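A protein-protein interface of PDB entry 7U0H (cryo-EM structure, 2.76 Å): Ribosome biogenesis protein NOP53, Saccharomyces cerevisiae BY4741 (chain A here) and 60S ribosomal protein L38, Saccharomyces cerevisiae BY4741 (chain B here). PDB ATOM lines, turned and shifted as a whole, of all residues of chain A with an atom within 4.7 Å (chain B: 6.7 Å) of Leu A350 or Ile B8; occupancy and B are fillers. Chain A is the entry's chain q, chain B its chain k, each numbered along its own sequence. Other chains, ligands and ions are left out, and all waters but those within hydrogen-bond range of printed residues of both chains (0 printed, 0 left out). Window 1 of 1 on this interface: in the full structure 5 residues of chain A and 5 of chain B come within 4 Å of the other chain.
O of Thr B6 is in hydrogen-bond range of NE of Arg A346 (3.0 Å).
The backbone NH of Lys B9 lies within hydrogen-bond range of the side-chain carboxylate of Asp B7 (3.0 Å).
OD2 of Asp B58 is in salt-bridge range of NZ of Lys B61, 3.0 Å away.
Among the printed residues, pairs that only touch across the chains: Leu A350 with Lys B61, Leu A350 with Ile B8, Val A353 with Lys B9, Ile A354 with Lys B64 and Val A347 with Lys B61.
Leu A350 touches just these residues of chain B: Ile B8 (3.5 Å) and Lys B61 (3.5 Å).
Ile B8 touches one residue of chain A.
Printed residues of chain B within 4 Å of Arg A346: Thr B6 (3.0 Å).
Of the printed residues of chain A, Lys B64 touches Ile A354.
Printed residues of chain B within 4 Å of Ile A354: Lys B64 (3.7 Å).
Printed residues of chain A within 4 Å of Lys B9: Val A353 (3.6 Å).
Of the printed residues of chain B, Val A347 touches Lys B61 (3.7 Å).
The nearest residue of chain B that does not touch Leu A350 is Ile B56 (4.8 Å).
Of the 9 printed residues of chain A, 5 touch a printed residue of chain B.
Among the printed residues, 6 pairs touch across the chains.
Among the printed residues, no Asp or Glu carboxylate lies within 4 Å of a Lys or Arg side-chain nitrogen of the other chain.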
ATOM      1  N   ARG A 346     -11.869  23.426 -21.466  1.00  0.00           N
ATOM      2  CA  ARG A 346     -10.910  22.568 -22.151  1.00  0.00           C
ATOM      3  C   ARG A 346     -11.449  21.151 -22.311  1.00  0.00           C
ATOM      4  O   ARG A 346     -11.215  20.502 -23.337  1.00  0.00           O
ATOM      5  CB  ARG A 346      -9.579  22.557 -21.405  1.00  0.00           C
ATOM      6  CG  ARG A 346      -8.547  21.620 -22.017  1.00  0.00           C
ATOM      7  CD  ARG A 346      -7.135  22.043 -21.669  1.00  0.00           C
ATOM      8  NE  ARG A 346      -6.810  23.355 -22.213  1.00  0.00           N
ATOM      9  CZ  ARG A 346      -6.815  24.483 -21.514  1.00  0.00           C
ATOM     10  NH1 ARG A 346      -7.109  24.494 -20.225  1.00  0.00           N
ATOM     11  NH2 ARG A 346      -6.511  25.626 -22.122  1.00  0.00           N
ATOM     12  N   VAL A 347     -12.170  20.652 -21.305  1.00  0.00           N
ATOM     13  CA  VAL A 347     -12.723  19.303 -21.388  1.00  0.00           C
ATOM     14  C   VAL A 347     -13.785  19.218 -22.478  1.00  0.00           C
ATOM     15  O   VAL A 347     -13.818  18.256 -23.256  1.00  0.00           O
ATOM     16  CB  VAL A 347     -13.282  18.869 -20.021  1.00  0.00           C
ATOM     17  CG1 VAL A 347     -14.164  17.639 -20.170  1.00  0.00           C
ATOM     18  CG2 VAL A 347     -12.152  18.590 -19.043  1.00  0.00           C
ATOM     19  N   LYS A 348     -14.662  20.222 -22.559  1.00  0.00           N
ATOM     20  CA  LYS A 348     -15.876  20.090 -23.364  1.00  0.00           C
ATOM     21  C   LYS A 348     -15.567  19.928 -24.848  1.00  0.00           C
ATOM     22  O   LYS A 348     -16.161  19.077 -25.519  1.00  0.00           O
ATOM     23  CB  LYS A 348     -16.785  21.297 -23.143  1.00  0.00           C
ATOM     24  CG  LYS A 348     -18.215  21.091 -23.610  1.00  0.00           C
ATOM     25  CD  LYS A 348     -18.923  20.056 -22.755  1.00  0.00           C
ATOM     26  CE  LYS A 348     -20.390  19.937 -23.127  1.00  0.00           C
ATOM     27  NZ  LYS A 348     -21.082  18.922 -22.284  1.00  0.00           N
ATOM     28  N   ASP A 349     -14.629  20.716 -25.374  1.00  0.00           N
ATOM     29  CA  ASP A 349     -14.424  20.801 -26.815  1.00  0.00           C
ATOM     30  C   ASP A 349     -13.849  19.525 -27.421  1.00  0.00           C
ATOM     31  O   ASP A 349     -13.756  19.437 -28.651  1.00  0.00           O
ATOM     32  CB  ASP A 349     -13.509  21.982 -27.141  1.00  0.00           C
ATOM     33  CG  ASP A 349     -13.553  22.369 -28.607  1.00  0.00           C
ATOM     34  OD1 ASP A 349     -14.571  22.076 -29.267  1.00  0.00           O
ATOM     35  OD2 ASP A 349     -12.567  22.957 -29.100  1.00  0.00           O
ATOM     36  N   LEU A 350     -13.432  18.558 -26.601  1.00  0.00           N
ATOM     37  CA  LEU A 350     -12.828  17.345 -27.148  1.00  0.00           C
ATOM     38  C   LEU A 350     -13.808  16.585 -28.031  1.00  0.00           C
ATOM     39  O   LEU A 350     -13.432  16.109 -29.107  1.00  0.00           O
ATOM     40  CB  LEU A 350     -12.313  16.452 -26.020  1.00  0.00           C
ATOM     41  CG  LEU A 350     -10.840  16.653 -25.651  1.00  0.00           C
ATOM     42  CD1 LEU A 350     -10.581  18.085 -25.249  1.00  0.00           C
ATOM     43  CD2 LEU A 350     -10.407  15.716 -24.541  1.00  0.00           C
ATOM     44  N   GLU A 351     -15.068  16.470 -27.607  1.00  0.00           N
ATOM     45  CA  GLU A 351     -16.053  15.785 -28.437  1.00  0.00           C
ATOM     46  C   GLU A 351     -16.221  16.489 -29.778  1.00  0.00           C
ATOM     47  O   GLU A 351     -16.228  15.841 -30.834  1.00  0.00           O
ATOM     48  CB  GLU A 351     -17.391  15.699 -27.701  1.00  0.00           C
ATOM     49  CG  GLU A 351     -17.321  14.982 -26.358  1.00  0.00           C
ATOM     50  CD  GLU A 351     -18.674  14.886 -25.668  1.00  0.00           C
ATOM     51  OE1 GLU A 351     -19.699  14.753 -26.368  1.00  0.00           O
ATOM     52  OE2 GLU A 351     -18.709  14.946 -24.420  1.00  0.00           O
ATOM     53  N   GLU A 352     -16.327  17.819 -29.757  1.00  0.00           N
ATOM     54  CA  GLU A 352     -16.532  18.571 -30.991  1.00  0.00           C
ATOM     55  C   GLU A 352     -15.342  18.435 -31.933  1.00  0.00           C
ATOM     56  O   GLU A 352     -15.516  18.293 -33.149  1.00  0.00           O
ATOM     57  CB  GLU A 352     -16.799  20.042 -30.668  1.00  0.00           C
ATOM     58  CG  GLU A 352     -16.967  20.930 -31.890  1.00  0.00           C
ATOM     59  CD  GLU A 352     -17.395  22.338 -31.532  1.00  0.00           C
ATOM     60  OE1 GLU A 352     -17.604  22.602 -30.328  1.00  0.00           O
ATOM     61  OE2 GLU A 352     -17.529  23.175 -32.449  1.00  0.00           O
ATOM     62  N   VAL A 353     -14.123  18.487 -31.395  1.00  0.00           N
ATOM     63  CA  VAL A 353     -12.943  18.392 -32.251  1.00  0.00           C
ATOM     64  C   VAL A 353     -12.776  16.974 -32.791  1.00  0.00           C
ATOM     65  O   VAL A 353     -12.374  16.782 -33.945  1.00  0.00           O
ATOM     66  CB  VAL A 353     -11.687  18.869 -31.501  1.00  0.00           C
ATOM     67  CG1 VAL A 353     -10.477  18.799 -32.412  1.00  0.00           C
ATOM     68  CG2 VAL A 353     -11.879  20.283 -30.989  1.00  0.00           C
ATOM     69  N   ILE A 354     -13.062  15.961 -31.968  1.00  0.00           N
ATOM     70  CA  ILE A 354     -12.961  14.578 -32.424  1.00  0.00           C
ATOM     71  C   ILE A 354     -13.972  14.303 -33.530  1.00  0.00           C
ATOM     72  O   ILE A 354     -13.679  13.582 -34.492  1.00  0.00           O
ATOM     73  CB  ILE A 354     -13.147  13.608 -31.242  1.00  0.00           C
ATOM     74  CG1 ILE A 354     -11.992  13.734 -30.248  1.00  0.00           C
ATOM     75  CG2 ILE A 354     -13.246  12.169 -31.738  1.00  0.00           C
ATOM     76  CD1 ILE A 354     -12.259  13.044 -28.918  1.00  0.00           C
ATOM     77  N   ILE B   5       1.492  21.888 -23.067  1.00  0.00           N
ATOM     78  CA  ILE B   5       0.544  22.444 -24.024  1.00  0.00           C
ATOM     79  C   ILE B   5      -0.864  22.081 -23.579  1.00  0.00           C
ATOM     80  O   ILE B   5      -1.119  20.951 -23.150  1.00  0.00           O
ATOM     81  CB  ILE B   5       0.821  21.956 -25.458  1.00  0.00           C
ATOM     82  CG1 ILE B   5       1.022  20.445 -25.486  1.00  0.00           C
ATOM     83  CG2 ILE B   5       2.035  22.665 -26.030  1.00  0.00           C
ATOM     84  CD1 ILE B   5       1.314  19.906 -26.860  1.00  0.00           C
ATOM     85  N   THR B   6      -1.776  23.047 -23.678  1.00  0.00           N
ATOM     86  CA  THR B   6      -3.134  22.917 -23.165  1.00  0.00           C
ATOM     87  C   THR B   6      -4.172  22.671 -24.255  1.00  0.00           C
ATOM     88  O   THR B   6      -5.029  21.799 -24.100  1.00  0.00           O
ATOM     89  CB  THR B   6      -3.515  24.173 -22.370  1.00  0.00           C
ATOM     90  OG1 THR B   6      -3.124  25.342 -23.100  1.00  0.00           O
ATOM     91  CG2 THR B   6      -2.833  24.177 -21.015  1.00  0.00           C
ATOM     92  N   ASP B   7      -4.119  23.421 -25.353  1.00  0.00           N
ATOM     93  CA  ASP B   7      -5.129  23.287 -26.394  1.00  0.00           C
ATOM     94  C   ASP B   7      -4.970  21.969 -27.139  1.00  0.00           C
ATOM     95  O   ASP B   7      -3.874  21.619 -27.589  1.00  0.00           O
ATOM     96  CB  ASP B   7      -5.045  24.454 -27.374  1.00  0.00           C
ATOM     97  CG  ASP B   7      -6.082  24.362 -28.485  1.00  0.00           C
ATOM     98  OD1 ASP B   7      -7.090  23.644 -28.309  1.00  0.00           O
ATOM     99  OD2 ASP B   7      -5.888  25.000 -29.540  1.00  0.00           O
ATOM    100  N   ILE B   8      -6.079  21.247 -27.289  1.00  0.00           N
ATOM    101  CA  ILE B   8      -6.064  19.996 -28.038  1.00  0.00           C
ATOM    102  C   ILE B   8      -5.816  20.257 -29.518  1.00  0.00           C
ATOM    103  O   ILE B   8      -5.131  19.481 -30.192  1.00  0.00           O
ATOM    104  CB  ILE B   8      -7.375  19.229 -27.794  1.00  0.00           C
ATOM    105  CG1 ILE B   8      -7.337  18.561 -26.423  1.00  0.00           C
ATOM    106  CG2 ILE B   8      -7.624  18.205 -28.882  1.00  0.00           C
ATOM    107  CD1 ILE B   8      -6.510  17.304 -26.387  1.00  0.00           C
ATOM    108  N   LYS B   9      -6.368  21.348 -30.050  1.00  0.00           N
ATOM    109  CA  LYS B   9      -6.108  21.698 -31.444  1.00  0.00           C
ATOM    110  C   LYS B   9      -4.628  21.977 -31.677  1.00  0.00           C
ATOM    111  O   LYS B   9      -4.051  21.526 -32.674  1.00  0.00           O
ATOM    112  CB  LYS B   9      -6.947  22.908 -31.844  1.00  0.00           C
ATOM    113  CG  LYS B   9      -8.435  22.651 -31.838  1.00  0.00           C
ATOM    114  CD  LYS B   9      -8.866  21.959 -33.112  1.00  0.00           C
ATOM    115  CE  LYS B   9     -10.303  22.303 -33.461  1.00  0.00           C
ATOM    116  NZ  LYS B   9     -10.728  21.650 -34.724  1.00  0.00           N
ATOM    117  N   GLN B  10      -4.002  22.728 -30.770  1.00  0.00           N
ATOM    118  CA  GLN B  10      -2.573  22.974 -30.888  1.00  0.00           C
ATOM    119  C   GLN B  10      -1.790  21.679 -30.745  1.00  0.00           C
ATOM    120  O   GLN B  10      -0.796  21.469 -31.445  1.00  0.00           O
ATOM    121  CB  GLN B  10      -2.118  23.998 -29.849  1.00  0.00           C
ATOM    122  CG  GLN B  10      -2.812  25.355 -29.950  1.00  0.00           C
ATOM    123  CD  GLN B  10      -2.573  26.051 -31.276  1.00  0.00           C
ATOM    124  OE1 GLN B  10      -1.617  26.812 -31.424  1.00  0.00           O
ATOM    125  NE2 GLN B  10      -3.446  25.797 -32.249  1.00  0.00           N
ATOM    126  N   PHE B  11      -2.235  20.789 -29.854  1.00  0.00           N
ATOM    127  CA  PHE B  11      -1.562  19.506 -29.694  1.00  0.00           C
ATOM    128  C   PHE B  11      -1.623  18.683 -30.974  1.00  0.00           C
ATOM    129  O   PHE B  11      -0.634  18.056 -31.363  1.00  0.00           O
ATOM    130  CB  PHE B  11      -2.169  18.725 -28.532  1.00  0.00           C
ATOM    131  CG  PHE B  11      -1.690  17.311 -28.450  1.00  0.00           C
ATOM    132  CD1 PHE B  11      -0.409  17.026 -28.018  1.00  0.00           C
ATOM    133  CD2 PHE B  11      -2.513  16.263 -28.821  1.00  0.00           C
ATOM    134  CE1 PHE B  11       0.038  15.726 -27.951  1.00  0.00           C
ATOM    135  CE2 PHE B  11      -2.070  14.964 -28.755  1.00  0.00           C
ATOM    136  CZ  PHE B  11      -0.793  14.697 -28.321  1.00  0.00           C
ATOM    137  N   LEU B  12      -2.773  18.679 -31.648  1.00  0.00           N
ATOM    138  CA  LEU B  12      -2.904  17.898 -32.875  1.00  0.00           C
ATOM    139  C   LEU B  12      -2.106  18.510 -34.020  1.00  0.00           C
ATOM    140  O   LEU B  12      -1.451  17.787 -34.783  1.00  0.00           O
ATOM    141  CB  LEU B  12      -4.377  17.752 -33.254  1.00  0.00           C
ATOM    142  CG  LEU B  12      -4.965  16.398 -32.852  1.00  0.00           C
ATOM    143  CD1 LEU B  12      -5.131  16.313 -31.348  1.00  0.00           C
ATOM    144  CD2 LEU B  12      -6.277  16.130 -33.566  1.00  0.00           C
ATOM    145  N   GLU B  13      -2.133  19.836 -34.159  1.00  0.00           N
ATOM    146  CA  GLU B  13      -1.302  20.468 -35.182  1.00  0.00           C
ATOM    147  C   GLU B  13       0.175  20.196 -34.926  1.00  0.00           C
ATOM    148  O   GLU B  13       0.942  19.928 -35.860  1.00  0.00           O
ATOM    149  CB  GLU B  13      -1.577  21.970 -35.227  1.00  0.00           C
ATOM    150  CG  GLU B  13      -3.014  22.315 -35.582  1.00  0.00           C
ATOM    151  CD  GLU B  13      -3.397  21.868 -36.982  1.00  0.00           C
ATOM    152  OE1 GLU B  13      -2.858  22.432 -37.956  1.00  0.00           O
ATOM    153  OE2 GLU B  13      -4.230  20.948 -37.107  1.00  0.00           O
ATOM    154  N   PHE B  43       0.505  12.750 -22.868  1.00  0.00           N
ATOM    155  CA  PHE B  43       0.967  12.594 -24.240  1.00  0.00           C
ATOM    156  C   PHE B  43       2.173  13.501 -24.432  1.00  0.00           C
ATOM    157  O   PHE B  43       2.056  14.723 -24.320  1.00  0.00           O
ATOM    158  CB  PHE B  43      -0.131  12.948 -25.243  1.00  0.00           C
ATOM    159  CG  PHE B  43      -1.425  12.223 -25.017  1.00  0.00           C
ATOM    160  CD1 PHE B  43      -2.375  12.725 -24.144  1.00  0.00           C
ATOM    161  CD2 PHE B  43      -1.700  11.050 -25.690  1.00  0.00           C
ATOM    162  CE1 PHE B  43      -3.568  12.062 -23.938  1.00  0.00           C
ATOM    163  CE2 PHE B  43      -2.890  10.386 -25.491  1.00  0.00           C
ATOM    164  CZ  PHE B  43      -3.824  10.892 -24.613  1.00  0.00           C
ATOM    165  N   LEU B  54       1.025  17.001 -22.900  1.00  0.00           N
ATOM    166  CA  LEU B  54      -0.393  17.278 -22.723  1.00  0.00           C
ATOM    167  C   LEU B  54      -0.934  16.331 -21.663  1.00  0.00           C
ATOM    168  O   LEU B  54      -0.790  15.112 -21.788  1.00  0.00           O
ATOM    169  CB  LEU B  54      -1.148  17.096 -24.038  1.00  0.00           C
ATOM    170  CG  LEU B  54      -2.671  17.054 -23.991  1.00  0.00           C
ATOM    171  CD1 LEU B  54      -3.235  18.413 -23.644  1.00  0.00           C
ATOM    172  CD2 LEU B  54      -3.211  16.558 -25.308  1.00  0.00           C
ATOM    173  N   ILE B  56      -4.076  14.781 -19.725  1.00  0.00           N
ATOM    174  CA  ILE B  56      -5.506  14.505 -19.761  1.00  0.00           C
ATOM    175  C   ILE B  56      -5.856  13.688 -18.526  1.00  0.00           C
ATOM    176  O   ILE B  56      -5.209  12.674 -18.242  1.00  0.00           O
ATOM    177  CB  ILE B  56      -5.910  13.752 -21.040  1.00  0.00           C
ATOM    178  CG1 ILE B  56      -5.477  14.531 -22.280  1.00  0.00           C
ATOM    179  CG2 ILE B  56      -7.409  13.513 -21.064  1.00  0.00           C
ATOM    180  CD1 ILE B  56      -6.150  15.876 -22.422  1.00  0.00           C
ATOM    181  N   ASP B  58      -8.999  12.447 -18.092  1.00  0.00           N
ATOM    182  CA  ASP B  58     -10.175  11.654 -18.439  1.00  0.00           C
ATOM    183  C   ASP B  58      -9.749  10.491 -19.323  1.00  0.00           C
ATOM    184  O   ASP B  58      -9.200  10.699 -20.412  1.00  0.00           O
ATOM    185  CB  ASP B  58     -11.224  12.512 -19.144  1.00  0.00           C
ATOM    186  CG  ASP B  58     -12.598  11.869 -19.149  1.00  0.00           C
ATOM    187  OD1 ASP B  58     -12.689  10.644 -19.373  1.00  0.00           O
ATOM    188  OD2 ASP B  58     -13.591  12.592 -18.920  1.00  0.00           O
ATOM    189  N   LYS B  61     -11.581  10.241 -22.896  1.00  0.00           N
ATOM    190  CA  LYS B  61     -11.052  11.260 -23.792  1.00  0.00           C
ATOM    191  C   LYS B  61      -9.634  10.926 -24.223  1.00  0.00           C
ATOM    192  O   LYS B  61      -9.267  11.126 -25.387  1.00  0.00           O
ATOM    193  CB  LYS B  61     -11.107  12.625 -23.114  1.00  0.00           C
ATOM    194  CG  LYS B  61     -12.500  13.209 -23.100  1.00  0.00           C
ATOM    195  CD  LYS B  61     -12.713  14.162 -21.947  1.00  0.00           C
ATOM    196  CE  LYS B  61     -14.193  14.261 -21.632  1.00  0.00           C
ATOM    197  NZ  LYS B  61     -14.824  12.908 -21.622  1.00  0.00           N
ATOM    198  N   ALA B  62      -8.823  10.410 -23.299  1.00  0.00           N
ATOM    199  CA  ALA B  62      -7.471   9.997 -23.655  1.00  0.00           C
ATOM    200  C   ALA B  62      -7.489   8.887 -24.695  1.00  0.00           C
ATOM    201  O   ALA B  62      -6.707   8.910 -25.653  1.00  0.00           O
ATOM    202  CB  ALA B  62      -6.718   9.552 -22.404  1.00  0.00           C
ATOM    203  N   LYS B  64      -9.879   8.242 -26.895  1.00  0.00           N
ATOM    204  CA  LYS B  64     -10.353   8.749 -28.176  1.00  0.00           C
ATOM    205  C   LYS B  64      -9.288   9.598 -28.860  1.00  0.00           C
ATOM    206  O   LYS B  64      -9.153   9.568 -30.087  1.00  0.00           O
ATOM    207  CB  LYS B  64     -11.650   9.534 -27.982  1.00  0.00           C
ATOM    208  CG  LYS B  64     -12.620   9.399 -29.145  1.00  0.00           C
ATOM    209  CD  LYS B  64     -14.058   9.609 -28.690  1.00  0.00           C
ATOM    210  CE  LYS B  64     -15.016   9.564 -29.871  1.00  0.00           C
ATOM    211  NZ  LYS B  64     -14.856   8.312 -30.663  1.00  0.00           N
ATOM    212  N   LEU B  65      -8.505  10.346 -28.080  1.00  0.00           N
ATOM    213  CA  LEU B  65      -7.378  11.082 -28.646  1.00  0.00           C
ATOM    214  C   LEU B  65      -6.318  10.132 -29.192  1.00  0.00           C
ATOM    215  O   LEU B  65      -5.732  10.385 -30.254  1.00  0.00           O
ATOM    216  CB  LEU B  65      -6.781  12.005 -27.585  1.00  0.00           C
ATOM    217  CG  LEU B  65      -5.881  13.126 -28.093  1.00  0.00           C
ATOM    218  CD1 LEU B  65      -6.683  14.080 -28.955  1.00  0.00           C
ATOM    219  CD2 LEU B  65      -5.237  13.859 -26.934  1.00  0.00           C
